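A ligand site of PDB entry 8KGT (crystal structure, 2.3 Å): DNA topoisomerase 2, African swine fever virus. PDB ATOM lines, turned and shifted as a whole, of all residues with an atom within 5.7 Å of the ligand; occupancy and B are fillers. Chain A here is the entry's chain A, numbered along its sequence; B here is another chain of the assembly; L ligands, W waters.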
ATOM      1  N   GLU A  60       1.485  -1.180  21.494  1.00  0.00           N
ATOM      2  CA  GLU A  60       1.344  -2.507  22.073  1.00  0.00           C
ATOM      3  C   GLU A  60       1.335  -2.463  23.599  1.00  0.00           C
ATOM      4  O   GLU A  60       0.602  -3.231  24.236  1.00  0.00           O
ATOM      5  CB  GLU A  60       2.494  -3.421  21.623  1.00  0.00           C
ATOM      6  CG  GLU A  60       2.494  -3.777  20.142  1.00  0.00           C
ATOM      7  CD  GLU A  60       1.352  -4.679  19.698  1.00  0.00           C
ATOM      8  OE1 GLU A  60       1.199  -4.864  18.443  1.00  0.00           O
ATOM      9  OE2 GLU A  60       0.602  -5.153  20.594  1.00  0.00           O
ATOM     10  N   ILE A  61       2.154  -1.618  24.194  1.00  0.00           N
ATOM     11  CA  ILE A  61       2.220  -1.504  25.626  1.00  0.00           C
ATOM     12  C   ILE A  61       1.049  -0.694  26.160  1.00  0.00           C
ATOM     13  O   ILE A  61       0.504  -1.003  27.190  1.00  0.00           O
ATOM     14  CB  ILE A  61       3.546  -0.860  26.032  1.00  0.00           C
ATOM     15  CG1 ILE A  61       4.707  -1.769  25.647  1.00  0.00           C
ATOM     16  CG2 ILE A  61       3.581  -0.549  27.510  1.00  0.00           C
ATOM     17  CD1 ILE A  61       6.023  -1.041  25.464  1.00  0.00           C
ATOM     18  N   ASN A  64      -1.781  -3.057  26.115  1.00  0.00           N
ATOM     19  CA  ASN A  64      -1.679  -3.993  27.230  1.00  0.00           C
ATOM     20  C   ASN A  64      -2.236  -3.360  28.505  1.00  0.00           C
ATOM     21  O   ASN A  64      -2.866  -4.040  29.300  1.00  0.00           O
ATOM     22  CB  ASN A  64      -0.257  -4.472  27.468  1.00  0.00           C
ATOM     23  CG  ASN A  64       0.218  -5.450  26.415  1.00  0.00           C
ATOM     24  OD1 ASN A  64      -0.592  -5.976  25.648  1.00  0.00           O
ATOM     25  ND2 ASN A  64       1.519  -5.689  26.372  1.00  0.00           N
ATOM     26  N   ALA A  65      -2.000  -2.066  28.705  1.00  0.00           N
ATOM     27  CA  ALA A  65      -2.429  -1.396  29.906  1.00  0.00           C
ATOM     28  C   ALA A  65      -3.944  -1.190  29.883  1.00  0.00           C
ATOM     29  O   ALA A  65      -4.588  -1.396  30.907  1.00  0.00           O
ATOM     30  CB  ALA A  65      -1.702  -0.084  30.071  1.00  0.00           C
ATOM     31  N   ASP A  67      -6.072  -3.030  28.227  1.00  0.00           N
ATOM     32  CA  ASP A  67      -6.612  -4.373  28.399  1.00  0.00           C
ATOM     33  C   ASP A  67      -6.725  -4.735  29.886  1.00  0.00           C
ATOM     34  O   ASP A  67      -7.716  -5.343  30.304  1.00  0.00           O
ATOM     35  CB  ASP A  67      -5.748  -5.424  27.709  1.00  0.00           C
ATOM     36  CG  ASP A  67      -5.912  -5.522  26.193  1.00  0.00           C
ATOM     37  OD1 ASP A  67      -6.805  -4.849  25.635  1.00  0.00           O
ATOM     38  OD2 ASP A  67      -5.131  -6.266  25.588  1.00  0.00           O
ATOM     39  N   HIS A  68      -5.689  -4.419  30.667  1.00  0.00           N
ATOM     40  CA  HIS A  68      -5.687  -4.719  32.091  1.00  0.00           C
ATOM     41  C   HIS A  68      -6.776  -3.897  32.797  1.00  0.00           C
ATOM     42  O   HIS A  68      -7.413  -4.371  33.737  1.00  0.00           O
ATOM     43  CB  HIS A  68      -4.296  -4.467  32.688  1.00  0.00           C
ATOM     44  CG  HIS A  68      -4.080  -5.159  33.998  1.00  0.00           C
ATOM     45  ND1 HIS A  68      -4.388  -6.489  34.202  1.00  0.00           N
ATOM     46  CD2 HIS A  68      -3.598  -4.711  35.164  1.00  0.00           C
ATOM     47  CE1 HIS A  68      -4.069  -6.814  35.439  1.00  0.00           C
ATOM     48  NE2 HIS A  68      -3.589  -5.743  36.048  1.00  0.00           N
ATOM     49  N   ASN A  95       0.850   1.145  35.028  1.00  0.00           N
ATOM     50  CA  ASN A  95      -0.529   1.008  35.468  1.00  0.00           C
ATOM     51  C   ASN A  95      -0.528   0.413  36.886  1.00  0.00           C
ATOM     52  O   ASN A  95       0.356  -0.349  37.237  1.00  0.00           O
ATOM     53  CB  ASN A  95      -1.330   0.201  34.450  1.00  0.00           C
ATOM     54  CG  ASN A  95      -0.882  -1.240  34.351  1.00  0.00           C
ATOM     55  OD1 ASN A  95      -0.210  -1.616  33.408  1.00  0.00           O
ATOM     56  ND2 ASN A  95      -1.244  -2.045  35.340  1.00  0.00           N
ATOM     57  N   PRO A  98      -3.744  -5.173  39.850  1.00  0.00           N
ATOM     58  CA  PRO A  98      -2.911  -6.366  40.055  1.00  0.00           C
ATOM     59  C   PRO A  98      -1.719  -6.385  39.099  1.00  0.00           C
ATOM     60  O   PRO A  98      -1.825  -5.992  37.939  1.00  0.00           O
ATOM     61  CB  PRO A  98      -3.879  -7.537  39.801  1.00  0.00           C
ATOM     62  CG  PRO A  98      -5.245  -6.949  40.162  1.00  0.00           C
ATOM     63  CD  PRO A  98      -5.173  -5.506  39.700  1.00  0.00           C
ATOM     64  N   GLY A  99      -0.568  -6.799  39.626  1.00  0.00           N
ATOM     65  CA  GLY A  99       0.633  -6.953  38.831  1.00  0.00           C
ATOM     66  C   GLY A  99       0.583  -8.202  37.961  1.00  0.00           C
ATOM     67  O   GLY A  99      -0.422  -8.926  37.945  1.00  0.00           O
ATOM     68  N   ILE A 100       1.646  -8.447  37.208  1.00  0.00           N
ATOM     69  CA  ILE A 100       1.783  -9.718  36.532  1.00  0.00           C
ATOM     70  C   ILE A 100       2.261 -10.739  37.565  1.00  0.00           C
ATOM     71  O   ILE A 100       3.235 -10.490  38.263  1.00  0.00           O
ATOM     72  CB  ILE A 100       2.757  -9.626  35.342  1.00  0.00           C
ATOM     73  CG1 ILE A 100       2.359  -8.515  34.359  1.00  0.00           C
ATOM     74  CG2 ILE A 100       2.851 -10.979  34.650  1.00  0.00           C
ATOM     75  CD1 ILE A 100       3.278  -8.354  33.189  1.00  0.00           C
ATOM     76  N   ALA A 122       5.849 -13.437  29.675  1.00  0.00           N
ATOM     77  CA  ALA A 122       5.078 -12.316  29.179  1.00  0.00           C
ATOM     78  C   ALA A 122       5.901 -11.415  28.258  1.00  0.00           C
ATOM     79  O   ALA A 122       5.343 -10.850  27.329  1.00  0.00           O
ATOM     80  CB  ALA A 122       4.530 -11.525  30.338  1.00  0.00           C
ATOM     81  N   ALA A 128       2.765 -15.943  23.318  1.00  0.00           N
ATOM     82  CA  ALA A 128       2.457 -16.313  24.689  1.00  0.00           C
ATOM     83  C   ALA A 128       1.811 -15.165  25.455  1.00  0.00           C
ATOM     84  O   ALA A 128       2.257 -14.020  25.392  1.00  0.00           O
ATOM     85  CB  ALA A 128       3.704 -16.781  25.400  1.00  0.00           C
ATOM     86  N   GLY A 129       0.790 -15.529  26.248  1.00  0.00           N
ATOM     87  CA  GLY A 129      -0.029 -14.596  26.987  1.00  0.00           C
ATOM     88  C   GLY A 129      -1.310 -15.261  27.464  1.00  0.00           C
ATOM     89  O   GLY A 129      -1.461 -16.477  27.381  1.00  0.00           O
ATOM     90  N   THR A 130      -2.244 -14.430  27.943  1.00  0.00           N
ATOM     91  CA  THR A 130      -3.478 -14.889  28.567  1.00  0.00           C
ATOM     92  C   THR A 130      -4.630 -14.823  27.574  1.00  0.00           C
ATOM     93  O   THR A 130      -5.770 -15.122  27.930  1.00  0.00           O
ATOM     94  CB  THR A 130      -3.766 -14.082  29.843  1.00  0.00           C
ATOM     95  OG1 THR A 130      -3.726 -12.698  29.486  1.00  0.00           O
ATOM     96  CG2 THR A 130      -2.757 -14.339  30.951  1.00  0.00           C
ATOM     97  N   ASN A 131      -4.338 -14.418  26.327  1.00  0.00           N
ATOM     98  CA  ASN A 131      -5.377 -14.256  25.329  1.00  0.00           C
ATOM     99  C   ASN A 131      -5.172 -15.216  24.158  1.00  0.00           C
ATOM    100  O   ASN A 131      -5.802 -15.033  23.121  1.00  0.00           O
ATOM    101  CB  ASN A 131      -5.431 -12.801  24.862  1.00  0.00           C
ATOM    102  CG  ASN A 131      -5.624 -11.844  26.014  1.00  0.00           C
ATOM    103  OD1 ASN A 131      -6.638 -11.924  26.717  1.00  0.00           O
ATOM    104  ND2 ASN A 131      -4.675 -10.933  26.204  1.00  0.00           N
ATOM    105  N   GLY A 141      -7.801  -5.928  23.200  1.00  0.00           N
ATOM    106  CA  GLY A 141      -7.023  -5.893  21.974  1.00  0.00           C
ATOM    107  C   GLY A 141      -6.026  -7.039  21.909  1.00  0.00           C
ATOM    108  O   GLY A 141      -5.766  -7.581  20.836  1.00  0.00           O
ATOM    109  N   GLY A 142      -5.495  -7.425  23.080  1.00  0.00           N
ATOM    110  CA  GLY A 142      -4.585  -8.550  23.206  1.00  0.00           C
ATOM    111  C   GLY A 142      -5.154  -9.832  22.611  1.00  0.00           C
ATOM    112  O   GLY A 142      -6.350 -10.111  22.722  1.00  0.00           O
ATOM    113  N   THR A 143      -4.279 -10.625  21.991  1.00  0.00           N
ATOM    114  CA  THR A 143      -4.695 -11.883  21.382  1.00  0.00           C
ATOM    115  C   THR A 143      -3.466 -12.682  20.956  1.00  0.00           C
ATOM    116  O   THR A 143      -3.436 -13.885  21.202  1.00  0.00           O
ATOM    117  CB  THR A 143      -5.718 -11.675  20.256  1.00  0.00           C
ATOM    118  OG1 THR A 143      -6.054 -12.961  19.754  1.00  0.00           O
ATOM    119  CG2 THR A 143      -5.224 -10.810  19.107  1.00  0.00           C
ATOM    120  N   ASN A 144      -2.458 -12.028  20.363  1.00  0.00           N
ATOM    121  CA  ASN A 144      -1.395 -12.724  19.667  1.00  0.00           C
ATOM    122  C   ASN A 144      -0.279 -13.175  20.595  1.00  0.00           C
ATOM    123  O   ASN A 144       0.459 -14.097  20.234  1.00  0.00           O
ATOM    124  CB  ASN A 144      -0.834 -11.898  18.507  1.00  0.00           C
ATOM    125  CG  ASN A 144      -1.884 -11.592  17.463  1.00  0.00           C
ATOM    126  OD1 ASN A 144      -2.702 -12.443  17.114  1.00  0.00           O
ATOM    127  ND2 ASN A 144      -1.913 -10.355  17.018  1.00  0.00           N
ATOM    128  N   GLY A 145      -0.149 -12.577  21.783  1.00  0.00           N
ATOM    129  CA  GLY A 145       0.962 -12.905  22.667  1.00  0.00           C
ATOM    130  C   GLY A 145       2.309 -12.542  22.019  1.00  0.00           C
ATOM    131  O   GLY A 145       3.268 -13.304  22.088  1.00  0.00           O
ATOM    132  N   VAL A 146       2.364 -11.335  21.439  1.00  0.00           N
ATOM    133  CA  VAL A 146       3.490 -10.943  20.607  1.00  0.00           C
ATOM    134  C   VAL A 146       3.877  -9.491  20.903  1.00  0.00           C
ATOM    135  O   VAL A 146       5.055  -9.183  20.910  1.00  0.00           O
ATOM    136  CB  VAL A 146       3.124 -11.222  19.136  1.00  0.00           C
ATOM    137  CG1 VAL A 146       3.239 -10.036  18.214  1.00  0.00           C
ATOM    138  CG2 VAL A 146       3.879 -12.430  18.599  1.00  0.00           C
ATOM    139  N   GLY A 147       2.888  -8.647  21.218  1.00  0.00           N
ATOM    140  CA  GLY A 147       3.080  -7.208  21.298  1.00  0.00           C
ATOM    141  C   GLY A 147       4.253  -6.788  22.173  1.00  0.00           C
ATOM    142  O   GLY A 147       5.028  -5.905  21.792  1.00  0.00           O
ATOM    143  N   LEU A 148       4.362  -7.381  23.366  1.00  0.00           N
ATOM    144  CA  LEU A 148       5.355  -6.966  24.342  1.00  0.00           C
ATOM    145  C   LEU A 148       6.729  -7.442  23.880  1.00  0.00           C
ATOM    146  O   LEU A 148       7.688  -6.715  24.053  1.00  0.00           O
ATOM    147  CB  LEU A 148       4.975  -7.474  25.738  1.00  0.00           C
ATOM    148  CG  LEU A 148       5.893  -7.044  26.903  1.00  0.00           C
ATOM    149  CD1 LEU A 148       6.063  -5.542  26.977  1.00  0.00           C
ATOM    150  CD2 LEU A 148       5.354  -7.542  28.237  1.00  0.00           C
ATOM    151  N   LYS A 149       6.816  -8.609  23.277  1.00  0.00           N
ATOM    152  CA  LYS A 149       8.061  -9.101  22.764  1.00  0.00           C
ATOM    153  C   LYS A 149       8.598  -8.256  21.598  1.00  0.00           C
ATOM    154  O   LYS A 149       9.802  -8.121  21.446  1.00  0.00           O
ATOM    155  CB  LYS A 149       7.899 -10.557  22.339  1.00  0.00           C
ATOM    156  CG  LYS A 149       8.069 -11.590  23.440  1.00  0.00           C
ATOM    157  CD  LYS A 149       6.907 -11.577  24.415  1.00  0.00           C
ATOM    158  CE  LYS A 149       5.585 -11.772  23.711  1.00  0.00           C
ATOM    159  NZ  LYS A 149       4.546 -12.261  24.667  1.00  0.00           N
ATOM    160  N   THR A 193       2.429  -2.490  37.307  1.00  0.00           N
ATOM    161  CA  THR A 193       3.349  -2.948  36.285  1.00  0.00           C
ATOM    162  C   THR A 193       3.891  -1.745  35.527  1.00  0.00           C
ATOM    163  O   THR A 193       3.119  -0.901  35.081  1.00  0.00           O
ATOM    164  CB  THR A 193       2.678  -3.925  35.306  1.00  0.00           C
ATOM    165  OG1 THR A 193       2.266  -5.054  36.072  1.00  0.00           O
ATOM    166  CG2 THR A 193       3.594  -4.361  34.189  1.00  0.00           C
ATOM    167  N   PHE B   4      -1.428 -18.149  31.580  1.00  0.00           N
ATOM    168  CA  PHE B   4      -0.388 -17.744  30.645  1.00  0.00           C
ATOM    169  C   PHE B   4       0.048 -18.927  29.785  1.00  0.00           C
ATOM    170  O   PHE B   4       0.872 -19.731  30.209  1.00  0.00           O
ATOM    171  CB  PHE B   4       0.828 -17.161  31.367  1.00  0.00           C
ATOM    172  CG  PHE B   4       0.708 -15.711  31.766  1.00  0.00           C
ATOM    173  CD1 PHE B   4      -0.033 -15.338  32.884  1.00  0.00           C
ATOM    174  CD2 PHE B   4       1.328 -14.722  31.014  1.00  0.00           C
ATOM    175  CE1 PHE B   4      -0.142 -14.002  33.240  1.00  0.00           C
ATOM    176  CE2 PHE B   4       1.211 -13.388  31.377  1.00  0.00           C
ATOM    177  CZ  PHE B   4       0.480 -13.027  32.486  1.00  0.00           C
HETATM  178  P1  LIG L   1      -1.247 -10.058  24.208  1.00  0.00           P
HETATM  179  O1  LIG L   1      -2.024 -10.938  25.129  1.00  0.00           O
HETATM  180  O2  LIG L   1      -1.451 -10.420  22.765  1.00  0.00           O
HETATM  181  O3  LIG L   1      -1.432  -8.598  24.496  1.00  0.00           O
HETATM  182  P2  LIG L   1       1.538  -9.516  24.881  1.00  0.00           P
HETATM  183  O4  LIG L   1       1.323  -8.071  24.553  1.00  0.00           O
HETATM  184  O5  LIG L   1       2.698 -10.240  24.297  1.00  0.00           O
HETATM  185  O6  LIG L   1       0.288 -10.396  24.472  1.00  0.00           O
HETATM  186  O7  LIG L   1       1.515  -9.690  26.479  1.00  0.00           O
HETATM  187  C1  LIG L   1       1.669 -10.993  27.075  1.00  0.00           C
HETATM  188  C2  LIG L   1       0.781 -11.071  28.296  1.00  0.00           C
HETATM  189  O8  LIG L   1       1.358 -10.289  29.368  1.00  0.00           O
HETATM  190  C3  LIG L   1      -0.633 -10.504  28.148  1.00  0.00           C
HETATM  191  O9  LIG L   1      -1.490 -11.461  27.532  1.00  0.00           O
HETATM  192  C4  LIG L   1      -1.006 -10.256  29.617  1.00  0.00           C
HETATM  193  O10 LIG L   1      -1.452 -11.438  30.242  1.00  0.00           O
HETATM  194  C5  LIG L   1       0.328  -9.818  30.224  1.00  0.00           C
HETATM  195  N1  LIG L   1       0.482  -8.381  30.371  1.00  0.00           N
HETATM  196  C6  LIG L   1       1.181  -7.523  29.558  1.00  0.00           C
HETATM  197  N2  LIG L   1       1.166  -6.277  29.969  1.00  0.00           N
HETATM  198  C7  LIG L   1       0.427  -6.312  31.145  1.00  0.00           C
HETATM  199  C8  LIG L   1       0.071  -5.318  32.075  1.00  0.00           C
HETATM  200  N3  LIG L   1       0.409  -4.041  31.954  1.00  0.00           N
HETATM  201  N4  LIG L   1      -0.664  -5.695  33.138  1.00  0.00           N
HETATM  202  C9  LIG L   1      -1.008  -6.988  33.263  1.00  0.00           C
HETATM  203  N5  LIG L   1      -0.729  -8.007  32.458  1.00  0.00           N
HETATM  204  C10 LIG L   1       0.012  -7.602  31.411  1.00  0.00           C
HETATM  205  O   HOH W   1       0.110  -9.552  20.856  1.00  0.00           O
HETATM  206  O   HOH W   2       1.493  -1.897  29.511  1.00  0.00           O
HETATM  207  O   HOH W   3      -3.126  -7.775  26.526  1.00  0.00           O
HETATM  208  O   HOH W   4      -0.277  -4.656  36.158  1.00  0.00           O
HETATM  209  O   HOH W   5      -0.054  -5.563  23.105  1.00  0.00           O
HETATM  210  O   HOH W   6      -2.075 -13.549  24.559  1.00  0.00           O
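Water W6 lies within hydrogen-bond range of an oxygen (O1) of the ligand (2.7 Å) and the backbone NH of Asn 131 (3.0 Å).
Water W3 lies within hydrogen-bond range of OD2 of Asp 67 (2.7 Å), O3 of the ligand (2.8 Å) and OD1 of Asn 64 (3.2 Å).
Water W5 lies within hydrogen-bond range of the side-chain carboxylate (OE2) of Glu 60, the side-chain amide oxygen (OD1) of Asn 64 and an oxygen (O4) of the ligand.
Water W4 lies within hydrogen-bond range of the side-chain hydroxyl (OG1) of Thr 193 (2.6 Å), the backbone carbonyl oxygen (O) of Pro 98 (2.7 Å), the side-chain amide nitrogen (ND2) of Asn 95 (2.9 Å), a nitrogen (N4) of the ligand (3.2 Å) and a ring nitrogen (NE2) of His 68 (3.5 Å).
Water W2 bridges the backbone carbonyl oxygen of Ile 61 and a nitrogen (N3) of the ligand.
ND1 of His 68 touches C9 of the ligand (3.5 Å).
CG1 of Ile 100 touches N5 of the ligand, 3.7 Å away.
CB of Ala 122 touches O8 of the ligand, at 3.5 Å.
O of Ala 128 touches C1 of the ligand (3.5 Å).
Gly 129 touches the ligand (CA to O9, 3.5 Å).
Gly 142 touches the ligand.
Thr 193 touches the ligand (CG2 to N3, 3.9 Å).
CZ of Phe 4 of chain B touches O10 of the ligand, 3.4 Å away.
Hydrophobic or aromatic side chains that line the ligand: His 68, Ile 100, Ala 122, Leu 148 and Phe 4 of chain B.
Within 4 Å of the ligand: Asn 64, His 68, Asn 95, Ile 100, Ala 122, Ala 128, Gly 129, Thr 130, Asn 131, Gly 142, Thr 143, Asn 144, Gly 145, Val 146, Gly 147, Leu 148, Lys 149, Thr 193 and Phe 4 of chain B.
Along chain A the residues within 4 Å of the ligand span positions 64 to 193.
An oxygen (O2) of the ligand sits at hydrogen-bond distance from the backbone NH (N) of Asn 144 (3.1 Å).
N of Thr 130 lies within hydrogen-bond range of O9 of the ligand (3.1 Å).
The side-chain amide nitrogen (ND2) of Asn 131 sits at hydrogen-bond distance from an oxygen (O1) of the ligand.
The backbone NH of Val 146 is in hydrogen-bond range of an oxygen (O5) of the ligand, at 3.1 Å.
The side-chain amide oxygen of Asn 95 is in hydrogen-bond range of a nitrogen (N3) of the ligand.
The side-chain amino group of Lys 149 is in salt-bridge range of an oxygen (O5) of the ligand, at 2.8 Å.
An oxygen (O5) of the ligand lies within hydrogen-bond range of the backbone NH (N) of Gly 147 (3.5 Å).
OG1 of Thr 130 lies within hydrogen-bond range of O10 of the ligand (2.7 Å).
N of Thr 143 is in hydrogen-bond range of O2 of the ligand, at 2.9 Å.
The backbone NH (N) of Gly 145 is in hydrogen-bond range of an oxygen (O2) of the ligand (2.7 Å).
OD1 of Asn 64 sits close to O3 of the ligand.
An oxygen (O4) of the ligand is in hydrogen-bond range of the backbone NH (N) of Leu 148 (3.3 Å).
O of Gly 145 is in hydrogen-bond range of NZ of Lys 149 (3.1 Å).
O of Gly 145 lies within hydrogen-bond range of N of Ala 128 (3.0 Å).
The side-chain amino group of Lys 149 sits at hydrogen-bond distance from the backbone carbonyl oxygen of Ala 128 (3.0 Å).
The side-chain amide oxygen of Asn 64 sits close to the backbone carbonyl oxygen of Glu 60 (3.3 Å).
NZ of Lys 149 sits at hydrogen-bond distance from O of Ala 122, 3.1 Å away.
The side-chain carboxylate of Asp 67 lies within hydrogen-bond range of the backbone NH of Gly 142 (2.8 Å).
A ring nitrogen (NE2) of His 68 is in hydrogen-bond range of the backbone carbonyl oxygen of Pro 98.
The backbone NH (N) of Thr 193 lies within hydrogen-bond range of the backbone carbonyl oxygen (O) of Asn 95 (3.0 Å).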
